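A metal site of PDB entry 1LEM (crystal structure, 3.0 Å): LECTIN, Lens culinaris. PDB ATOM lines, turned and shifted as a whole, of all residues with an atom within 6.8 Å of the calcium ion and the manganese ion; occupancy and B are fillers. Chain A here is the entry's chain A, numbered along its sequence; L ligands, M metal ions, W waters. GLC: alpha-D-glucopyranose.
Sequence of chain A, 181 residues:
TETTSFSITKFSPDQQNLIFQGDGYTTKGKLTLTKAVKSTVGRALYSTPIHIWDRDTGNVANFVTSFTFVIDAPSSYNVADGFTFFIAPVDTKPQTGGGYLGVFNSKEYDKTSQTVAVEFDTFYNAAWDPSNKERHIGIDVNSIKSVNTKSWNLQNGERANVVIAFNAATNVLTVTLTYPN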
ATOM      1  N   ASP A  81     -21.055  12.465  -5.730  1.00  0.00           N
ATOM      2  CA  ASP A  81     -20.151  11.536  -5.144  1.00  0.00           C
ATOM      3  C   ASP A  81     -18.727  11.905  -4.889  1.00  0.00           C
ATOM      4  O   ASP A  81     -18.003  11.179  -4.170  1.00  0.00           O
ATOM      5  CB  ASP A  81     -20.091  10.327  -6.067  1.00  0.00           C
ATOM      6  CG  ASP A  81     -20.841   9.126  -5.511  1.00  0.00           C
ATOM      7  OD1 ASP A  81     -20.389   8.502  -4.488  1.00  0.00           O
ATOM      8  OD2 ASP A  81     -21.934   8.739  -6.079  1.00  0.00           O
ATOM      9  N   GLY A  98     -19.508   5.944  -9.545  1.00  0.00           N
ATOM     10  CA  GLY A  98     -19.991   6.116  -8.180  1.00  0.00           C
ATOM     11  C   GLY A  98     -18.892   6.397  -7.140  1.00  0.00           C
ATOM     12  O   GLY A  98     -18.037   7.236  -7.369  1.00  0.00           O
ATOM     13  N   GLY A  99     -18.712   5.645  -6.054  1.00  0.00           N
ATOM     14  CA  GLY A  99     -17.732   5.959  -5.025  1.00  0.00           C
ATOM     15  C   GLY A  99     -16.292   5.812  -5.466  1.00  0.00           C
ATOM     16  O   GLY A  99     -15.449   6.216  -4.644  1.00  0.00           O
ATOM     17  N   TYR A 100     -16.024   5.174  -6.661  1.00  0.00           N
ATOM     18  CA  TYR A 100     -14.692   4.974  -7.262  1.00  0.00           C
ATOM     19  C   TYR A 100     -14.226   6.199  -8.067  1.00  0.00           C
ATOM     20  O   TYR A 100     -13.068   6.305  -8.516  1.00  0.00           O
ATOM     21  CB  TYR A 100     -14.683   3.748  -8.181  1.00  0.00           C
ATOM     22  CG  TYR A 100     -14.714   2.446  -7.408  1.00  0.00           C
ATOM     23  CD1 TYR A 100     -13.637   2.080  -6.591  1.00  0.00           C
ATOM     24  CD2 TYR A 100     -15.819   1.619  -7.491  1.00  0.00           C
ATOM     25  CE1 TYR A 100     -13.674   0.896  -5.864  1.00  0.00           C
ATOM     26  CE2 TYR A 100     -15.871   0.426  -6.760  1.00  0.00           C
ATOM     27  CZ  TYR A 100     -14.800   0.047  -5.940  1.00  0.00           C
ATOM     28  OH  TYR A 100     -14.837  -1.161  -5.216  1.00  0.00           O
ATOM     29  N   LEU A 101     -15.196   7.143  -8.237  1.00  0.00           N
ATOM     30  CA  LEU A 101     -15.022   8.516  -8.712  1.00  0.00           C
ATOM     31  C   LEU A 101     -14.509   8.589 -10.120  1.00  0.00           C
ATOM     32  O   LEU A 101     -13.817   9.564 -10.471  1.00  0.00           O
ATOM     33  CB  LEU A 101     -14.054   9.258  -7.762  1.00  0.00           C
ATOM     34  CG  LEU A 101     -14.426   9.438  -6.325  1.00  0.00           C
ATOM     35  CD1 LEU A 101     -13.409  10.268  -5.585  1.00  0.00           C
ATOM     36  CD2 LEU A 101     -15.747  10.165  -6.286  1.00  0.00           C
ATOM     37  N   GLU A 119      -8.620  13.767  -4.064  1.00  0.00           N
ATOM     38  CA  GLU A 119     -10.060  13.702  -4.129  1.00  0.00           C
ATOM     39  C   GLU A 119     -10.689  14.575  -3.063  1.00  0.00           C
ATOM     40  O   GLU A 119     -10.075  14.964  -2.051  1.00  0.00           O
ATOM     41  CB  GLU A 119     -10.490  12.258  -3.959  1.00  0.00           C
ATOM     42  CG  GLU A 119      -9.679  11.529  -2.855  1.00  0.00           C
ATOM     43  CD  GLU A 119     -10.279  10.273  -2.224  1.00  0.00           C
ATOM     44  OE1 GLU A 119     -10.465   9.232  -2.880  1.00  0.00           O
ATOM     45  OE2 GLU A 119     -10.512  10.332  -1.019  1.00  0.00           O
ATOM     46  N   ASP A 121     -14.063  14.004  -1.500  1.00  0.00           N
ATOM     47  CA  ASP A 121     -15.071  12.942  -1.332  1.00  0.00           C
ATOM     48  C   ASP A 121     -16.222  13.372  -0.458  1.00  0.00           C
ATOM     49  O   ASP A 121     -15.976  13.737   0.713  1.00  0.00           O
ATOM     50  CB  ASP A 121     -14.478  11.689  -0.719  1.00  0.00           C
ATOM     51  CG  ASP A 121     -15.370  10.417  -0.831  1.00  0.00           C
ATOM     52  OD1 ASP A 121     -16.558  10.472  -1.194  1.00  0.00           O
ATOM     53  OD2 ASP A 121     -14.830   9.340  -0.605  1.00  0.00           O
ATOM     54  N   THR A 122     -17.425  13.225  -1.013  1.00  0.00           N
ATOM     55  CA  THR A 122     -18.614  13.776  -0.369  1.00  0.00           C
ATOM     56  C   THR A 122     -19.544  12.717   0.163  1.00  0.00           C
ATOM     57  O   THR A 122     -20.644  12.991   0.659  1.00  0.00           O
ATOM     58  CB  THR A 122     -19.515  14.728  -1.323  1.00  0.00           C
ATOM     59  OG1 THR A 122     -19.801  14.079  -2.574  1.00  0.00           O
ATOM     60  CG2 THR A 122     -18.857  16.079  -1.536  1.00  0.00           C
ATOM     61  N   PHE A 123     -19.063  11.492   0.080  1.00  0.00           N
ATOM     62  CA  PHE A 123     -19.910  10.371   0.431  1.00  0.00           C
ATOM     63  C   PHE A 123     -19.094   9.185   0.898  1.00  0.00           C
ATOM     64  O   PHE A 123     -18.173   8.746   0.170  1.00  0.00           O
ATOM     65  CB  PHE A 123     -20.672  10.103  -0.805  1.00  0.00           C
ATOM     66  CG  PHE A 123     -21.633   9.008  -0.590  1.00  0.00           C
ATOM     67  CD1 PHE A 123     -22.881   9.357  -0.144  1.00  0.00           C
ATOM     68  CD2 PHE A 123     -21.302   7.707  -0.902  1.00  0.00           C
ATOM     69  CE1 PHE A 123     -23.825   8.366   0.009  1.00  0.00           C
ATOM     70  CE2 PHE A 123     -22.250   6.727  -0.744  1.00  0.00           C
ATOM     71  CZ  PHE A 123     -23.508   7.056  -0.300  1.00  0.00           C
ATOM     72  N   TYR A 124     -19.487   8.714   2.134  1.00  0.00           N
ATOM     73  CA  TYR A 124     -18.821   7.584   2.803  1.00  0.00           C
ATOM     74  C   TYR A 124     -19.219   6.231   2.212  1.00  0.00           C
ATOM     75  O   TYR A 124     -20.367   5.762   2.169  1.00  0.00           O
ATOM     76  CB  TYR A 124     -19.118   7.552   4.383  1.00  0.00           C
ATOM     77  CG  TYR A 124     -18.542   6.406   5.289  1.00  0.00           C
ATOM     78  CD1 TYR A 124     -17.202   6.382   5.699  1.00  0.00           C
ATOM     79  CD2 TYR A 124     -19.357   5.333   5.735  1.00  0.00           C
ATOM     80  CE1 TYR A 124     -16.709   5.364   6.528  1.00  0.00           C
ATOM     81  CE2 TYR A 124     -18.873   4.319   6.565  1.00  0.00           C
ATOM     82  CZ  TYR A 124     -17.536   4.321   6.943  1.00  0.00           C
ATOM     83  OH  TYR A 124     -17.009   3.293   7.723  1.00  0.00           O
ATOM     84  N   ASN A 125     -18.147   5.591   1.777  1.00  0.00           N
ATOM     85  CA  ASN A 125     -18.222   4.281   1.221  1.00  0.00           C
ATOM     86  C   ASN A 125     -17.499   3.596   2.349  1.00  0.00           C
ATOM     87  O   ASN A 125     -16.323   3.786   2.699  1.00  0.00           O
ATOM     88  CB  ASN A 125     -17.473   4.264  -0.071  1.00  0.00           C
ATOM     89  CG  ASN A 125     -18.174   5.083  -1.158  1.00  0.00           C
ATOM     90  OD1 ASN A 125     -17.890   6.247  -1.484  1.00  0.00           O
ATOM     91  ND2 ASN A 125     -19.130   4.369  -1.730  1.00  0.00           N
ATOM     92  N   TRP A 128     -14.067   1.612   2.492  1.00  0.00           N
ATOM     93  CA  TRP A 128     -12.701   2.136   2.296  1.00  0.00           C
ATOM     94  C   TRP A 128     -12.529   3.544   2.812  1.00  0.00           C
ATOM     95  O   TRP A 128     -11.402   4.031   2.994  1.00  0.00           O
ATOM     96  CB  TRP A 128     -12.265   2.163   0.786  1.00  0.00           C
ATOM     97  CG  TRP A 128     -13.180   2.886  -0.232  1.00  0.00           C
ATOM     98  CD1 TRP A 128     -13.371   4.250  -0.202  1.00  0.00           C
ATOM     99  CD2 TRP A 128     -13.965   2.277  -1.186  1.00  0.00           C
ATOM    100  NE1 TRP A 128     -14.304   4.513  -1.096  1.00  0.00           N
ATOM    101  CE2 TRP A 128     -14.703   3.356  -1.695  1.00  0.00           C
ATOM    102  CE3 TRP A 128     -14.211   1.015  -1.681  1.00  0.00           C
ATOM    103  CZ2 TRP A 128     -15.654   3.194  -2.694  1.00  0.00           C
ATOM    104  CZ3 TRP A 128     -15.172   0.857  -2.679  1.00  0.00           C
ATOM    105  CH2 TRP A 128     -15.891   1.928  -3.190  1.00  0.00           C
ATOM    106  N   ASP A 129     -13.647   4.247   2.991  1.00  0.00           N
ATOM    107  CA  ASP A 129     -13.541   5.643   3.368  1.00  0.00           C
ATOM    108  C   ASP A 129     -13.353   5.676   4.870  1.00  0.00           C
ATOM    109  O   ASP A 129     -13.807   4.730   5.543  1.00  0.00           O
ATOM    110  CB  ASP A 129     -14.816   6.429   2.901  1.00  0.00           C
ATOM    111  CG  ASP A 129     -14.794   6.943   1.436  1.00  0.00           C
ATOM    112  OD1 ASP A 129     -13.723   7.179   0.875  1.00  0.00           O
ATOM    113  OD2 ASP A 129     -15.845   7.119   0.825  1.00  0.00           O
ATOM    114  N   PRO A 130     -12.700   6.696   5.450  1.00  0.00           N
ATOM    115  CA  PRO A 130     -12.510   6.871   6.886  1.00  0.00           C
ATOM    116  C   PRO A 130     -13.770   6.621   7.682  1.00  0.00           C
ATOM    117  O   PRO A 130     -14.809   7.295   7.508  1.00  0.00           O
ATOM    118  CB  PRO A 130     -12.078   8.278   7.172  1.00  0.00           C
ATOM    119  CG  PRO A 130     -11.515   8.681   5.850  1.00  0.00           C
ATOM    120  CD  PRO A 130     -12.437   8.002   4.852  1.00  0.00           C
ATOM    121  N   HIS A 136     -14.030  14.538   3.212  1.00  0.00           N
ATOM    122  CA  HIS A 136     -12.587  14.605   3.290  1.00  0.00           C
ATOM    123  C   HIS A 136     -11.879  14.862   1.985  1.00  0.00           C
ATOM    124  O   HIS A 136     -12.417  14.535   0.906  1.00  0.00           O
ATOM    125  CB  HIS A 136     -12.110  13.292   3.906  1.00  0.00           C
ATOM    126  CG  HIS A 136     -12.600  12.076   3.121  1.00  0.00           C
ATOM    127  ND1 HIS A 136     -13.789  11.479   3.230  1.00  0.00           N
ATOM    128  CD2 HIS A 136     -11.875  11.365   2.151  1.00  0.00           C
ATOM    129  CE1 HIS A 136     -13.805  10.470   2.384  1.00  0.00           C
ATOM    130  NE2 HIS A 136     -12.656  10.391   1.733  1.00  0.00           N
ATOM    131  N   GLY A 138      -8.507  13.683   0.139  1.00  0.00           N
ATOM    132  CA  GLY A 138      -7.618  12.550   0.258  1.00  0.00           C
ATOM    133  C   GLY A 138      -6.627  12.525  -0.926  1.00  0.00           C
ATOM    134  O   GLY A 138      -6.936  13.041  -2.017  1.00  0.00           O
ATOM    135  N   ASP A 140      -4.652   9.671  -3.180  1.00  0.00           N
ATOM    136  CA  ASP A 140      -4.690   8.240  -3.411  1.00  0.00           C
ATOM    137  C   ASP A 140      -3.703   7.917  -4.497  1.00  0.00           C
ATOM    138  O   ASP A 140      -3.498   8.661  -5.485  1.00  0.00           O
ATOM    139  CB  ASP A 140      -5.895   7.693  -4.028  1.00  0.00           C
ATOM    140  CG  ASP A 140      -7.138   8.458  -3.748  1.00  0.00           C
ATOM    141  OD1 ASP A 140      -7.223   9.132  -2.738  1.00  0.00           O
ATOM    142  OD2 ASP A 140      -8.038   8.363  -4.563  1.00  0.00           O
ATOM    143  N   ILE A 144      -8.563   3.245  -4.763  1.00  0.00           N
ATOM    144  CA  ILE A 144      -9.554   4.150  -4.195  1.00  0.00           C
ATOM    145  C   ILE A 144      -9.453   4.427  -2.686  1.00  0.00           C
ATOM    146  O   ILE A 144     -10.166   5.266  -2.123  1.00  0.00           O
ATOM    147  CB  ILE A 144     -10.946   3.632  -4.527  1.00  0.00           C
ATOM    148  CG1 ILE A 144     -11.977   4.767  -4.358  1.00  0.00           C
ATOM    149  CG2 ILE A 144     -11.285   2.488  -3.612  1.00  0.00           C
ATOM    150  CD1 ILE A 144     -11.927   5.988  -5.311  1.00  0.00           C
ATOM    151  N   LYS A 145      -8.587   3.701  -1.978  1.00  0.00           N
ATOM    152  CA  LYS A 145      -8.298   3.906  -0.565  1.00  0.00           C
ATOM    153  C   LYS A 145      -7.242   4.968  -0.305  1.00  0.00           C
ATOM    154  O   LYS A 145      -6.054   4.685  -0.482  1.00  0.00           O
ATOM    155  CB  LYS A 145      -7.825   2.578  -0.019  1.00  0.00           C
ATOM    156  CG  LYS A 145      -8.776   1.917   0.964  1.00  0.00           C
ATOM    157  CD  LYS A 145      -8.381   2.282   2.376  1.00  0.00           C
ATOM    158  CE  LYS A 145      -7.165   1.429   2.682  1.00  0.00           C
ATOM    159  NZ  LYS A 145      -6.132   2.186   3.379  1.00  0.00           N
ATOM    160  N   SER A 146      -7.570   6.184   0.085  1.00  0.00           N
ATOM    161  CA  SER A 146      -6.539   7.190   0.256  1.00  0.00           C
ATOM    162  C   SER A 146      -5.401   6.788   1.169  1.00  0.00           C
ATOM    163  O   SER A 146      -5.600   6.207   2.226  1.00  0.00           O
ATOM    164  CB  SER A 146      -7.078   8.478   0.834  1.00  0.00           C
ATOM    165  OG  SER A 146      -8.440   8.642   0.450  1.00  0.00           O
ATOM    166  N   THR A 149      -5.648  11.381   4.444  1.00  0.00           N
ATOM    167  CA  THR A 149      -6.871  12.161   4.354  1.00  0.00           C
ATOM    168  C   THR A 149      -6.851  13.332   5.363  1.00  0.00           C
ATOM    169  O   THR A 149      -5.999  13.416   6.283  1.00  0.00           O
ATOM    170  CB  THR A 149      -8.171  11.303   4.624  1.00  0.00           C
ATOM    171  OG1 THR A 149      -7.905  10.772   5.878  1.00  0.00           O
ATOM    172  CG2 THR A 149      -8.506  10.115   3.741  1.00  0.00           C
HETATM  173  C1  GLC L   1     -24.380   3.795  -5.223  1.00  0.00           C
HETATM  174  C2  GLC L   1     -22.978   3.432  -5.819  1.00  0.00           C
HETATM  175  C3  GLC L   1     -21.822   3.931  -4.859  1.00  0.00           C
HETATM  176  C4  GLC L   1     -21.973   5.429  -4.617  1.00  0.00           C
HETATM  177  C5  GLC L   1     -23.310   5.743  -3.945  1.00  0.00           C
HETATM  178  C6  GLC L   1     -23.596   7.312  -3.719  1.00  0.00           C
HETATM  179  O1  GLC L   1     -24.554   2.884  -4.083  1.00  0.00           O
HETATM  180  O2  GLC L   1     -22.893   2.012  -5.878  1.00  0.00           O
HETATM  181  O3  GLC L   1     -20.499   3.626  -5.311  1.00  0.00           O
HETATM  182  O4  GLC L   1     -20.918   5.837  -3.792  1.00  0.00           O
HETATM  183  O5  GLC L   1     -24.369   5.184  -4.783  1.00  0.00           O
HETATM  184  O6  GLC L   1     -24.285   7.983  -4.778  1.00  0.00           O
HETATM  185 CA    CA M   1     -16.472   7.811  -1.514  1.00  0.00          CA
HETATM  186 MN    MN M   2     -12.498   8.658  -0.009  1.00  0.00          MN
HETATM  187  O   HOH W   1     -10.395   7.387   1.790  1.00  0.00           O
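The side-chain amide nitrogen of Asn 125 lies within hydrogen-bond range of an oxygen (O4) of the ligand.
The backbone NH (N) of Gly 99 lies within hydrogen-bond range of an oxygen (O3) of the ligand.
OD2 of Asp 81 is in hydrogen-bond range of O6 of the ligand, at 2.8 Å.
The side-chain carboxylate (OD1) of Asp 129 sits close to the indole nitrogen (NE1) of Trp 128, 3.4 Å away.
OE2 of Glu 119 sits close to NE2 of His 136.
The side-chain carboxylate of Glu 119 is in hydrogen-bond range of the side-chain hydroxyl of Ser 146 (3.1 Å).
O of Gly 138 lies within hydrogen-bond range of N of Glu 119 (2.7 Å).
O of Gly 99 touches the calcium ion, at 3.7 Å.
NE1 of Trp 128 touches the calcium ion, 3.97 Å away.
Of the 21 residues printed, 6 come within 4 Å of the calcium ion.
The nearest printed residue that does not touch the calcium ion is Asp 81 (4.6 Å).
Within 4 Å of the manganese ion: Glu 119, Asp 121, Asp 129 and His 136.
Along chain A the residues within 4 Å of the manganese ion span positions 119 to 136.
The calcium ion is bound by the side-chain amide oxygen (OD1) of Asn 125, the side-chain carboxylate (OD2) of Asp 121, the side-chain carboxylate (OD2) of Asp 129, the backbone carbonyl oxygen (O) of Phe 123 and the side-chain carboxylate (OD1) of Asp 121.
The calcium ion has five donor atoms within binding distance.
The manganese ion is bound by OD1 of Asp 129.
The manganese ion is bound by a ring nitrogen (NE2) of His 136 (2.5 Å).
OD2 of Asp 121 binds the manganese ion, at 2.5 Å.
Slightly farther from the manganese ion lies OE2 of Glu 119 (2.8 Å).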
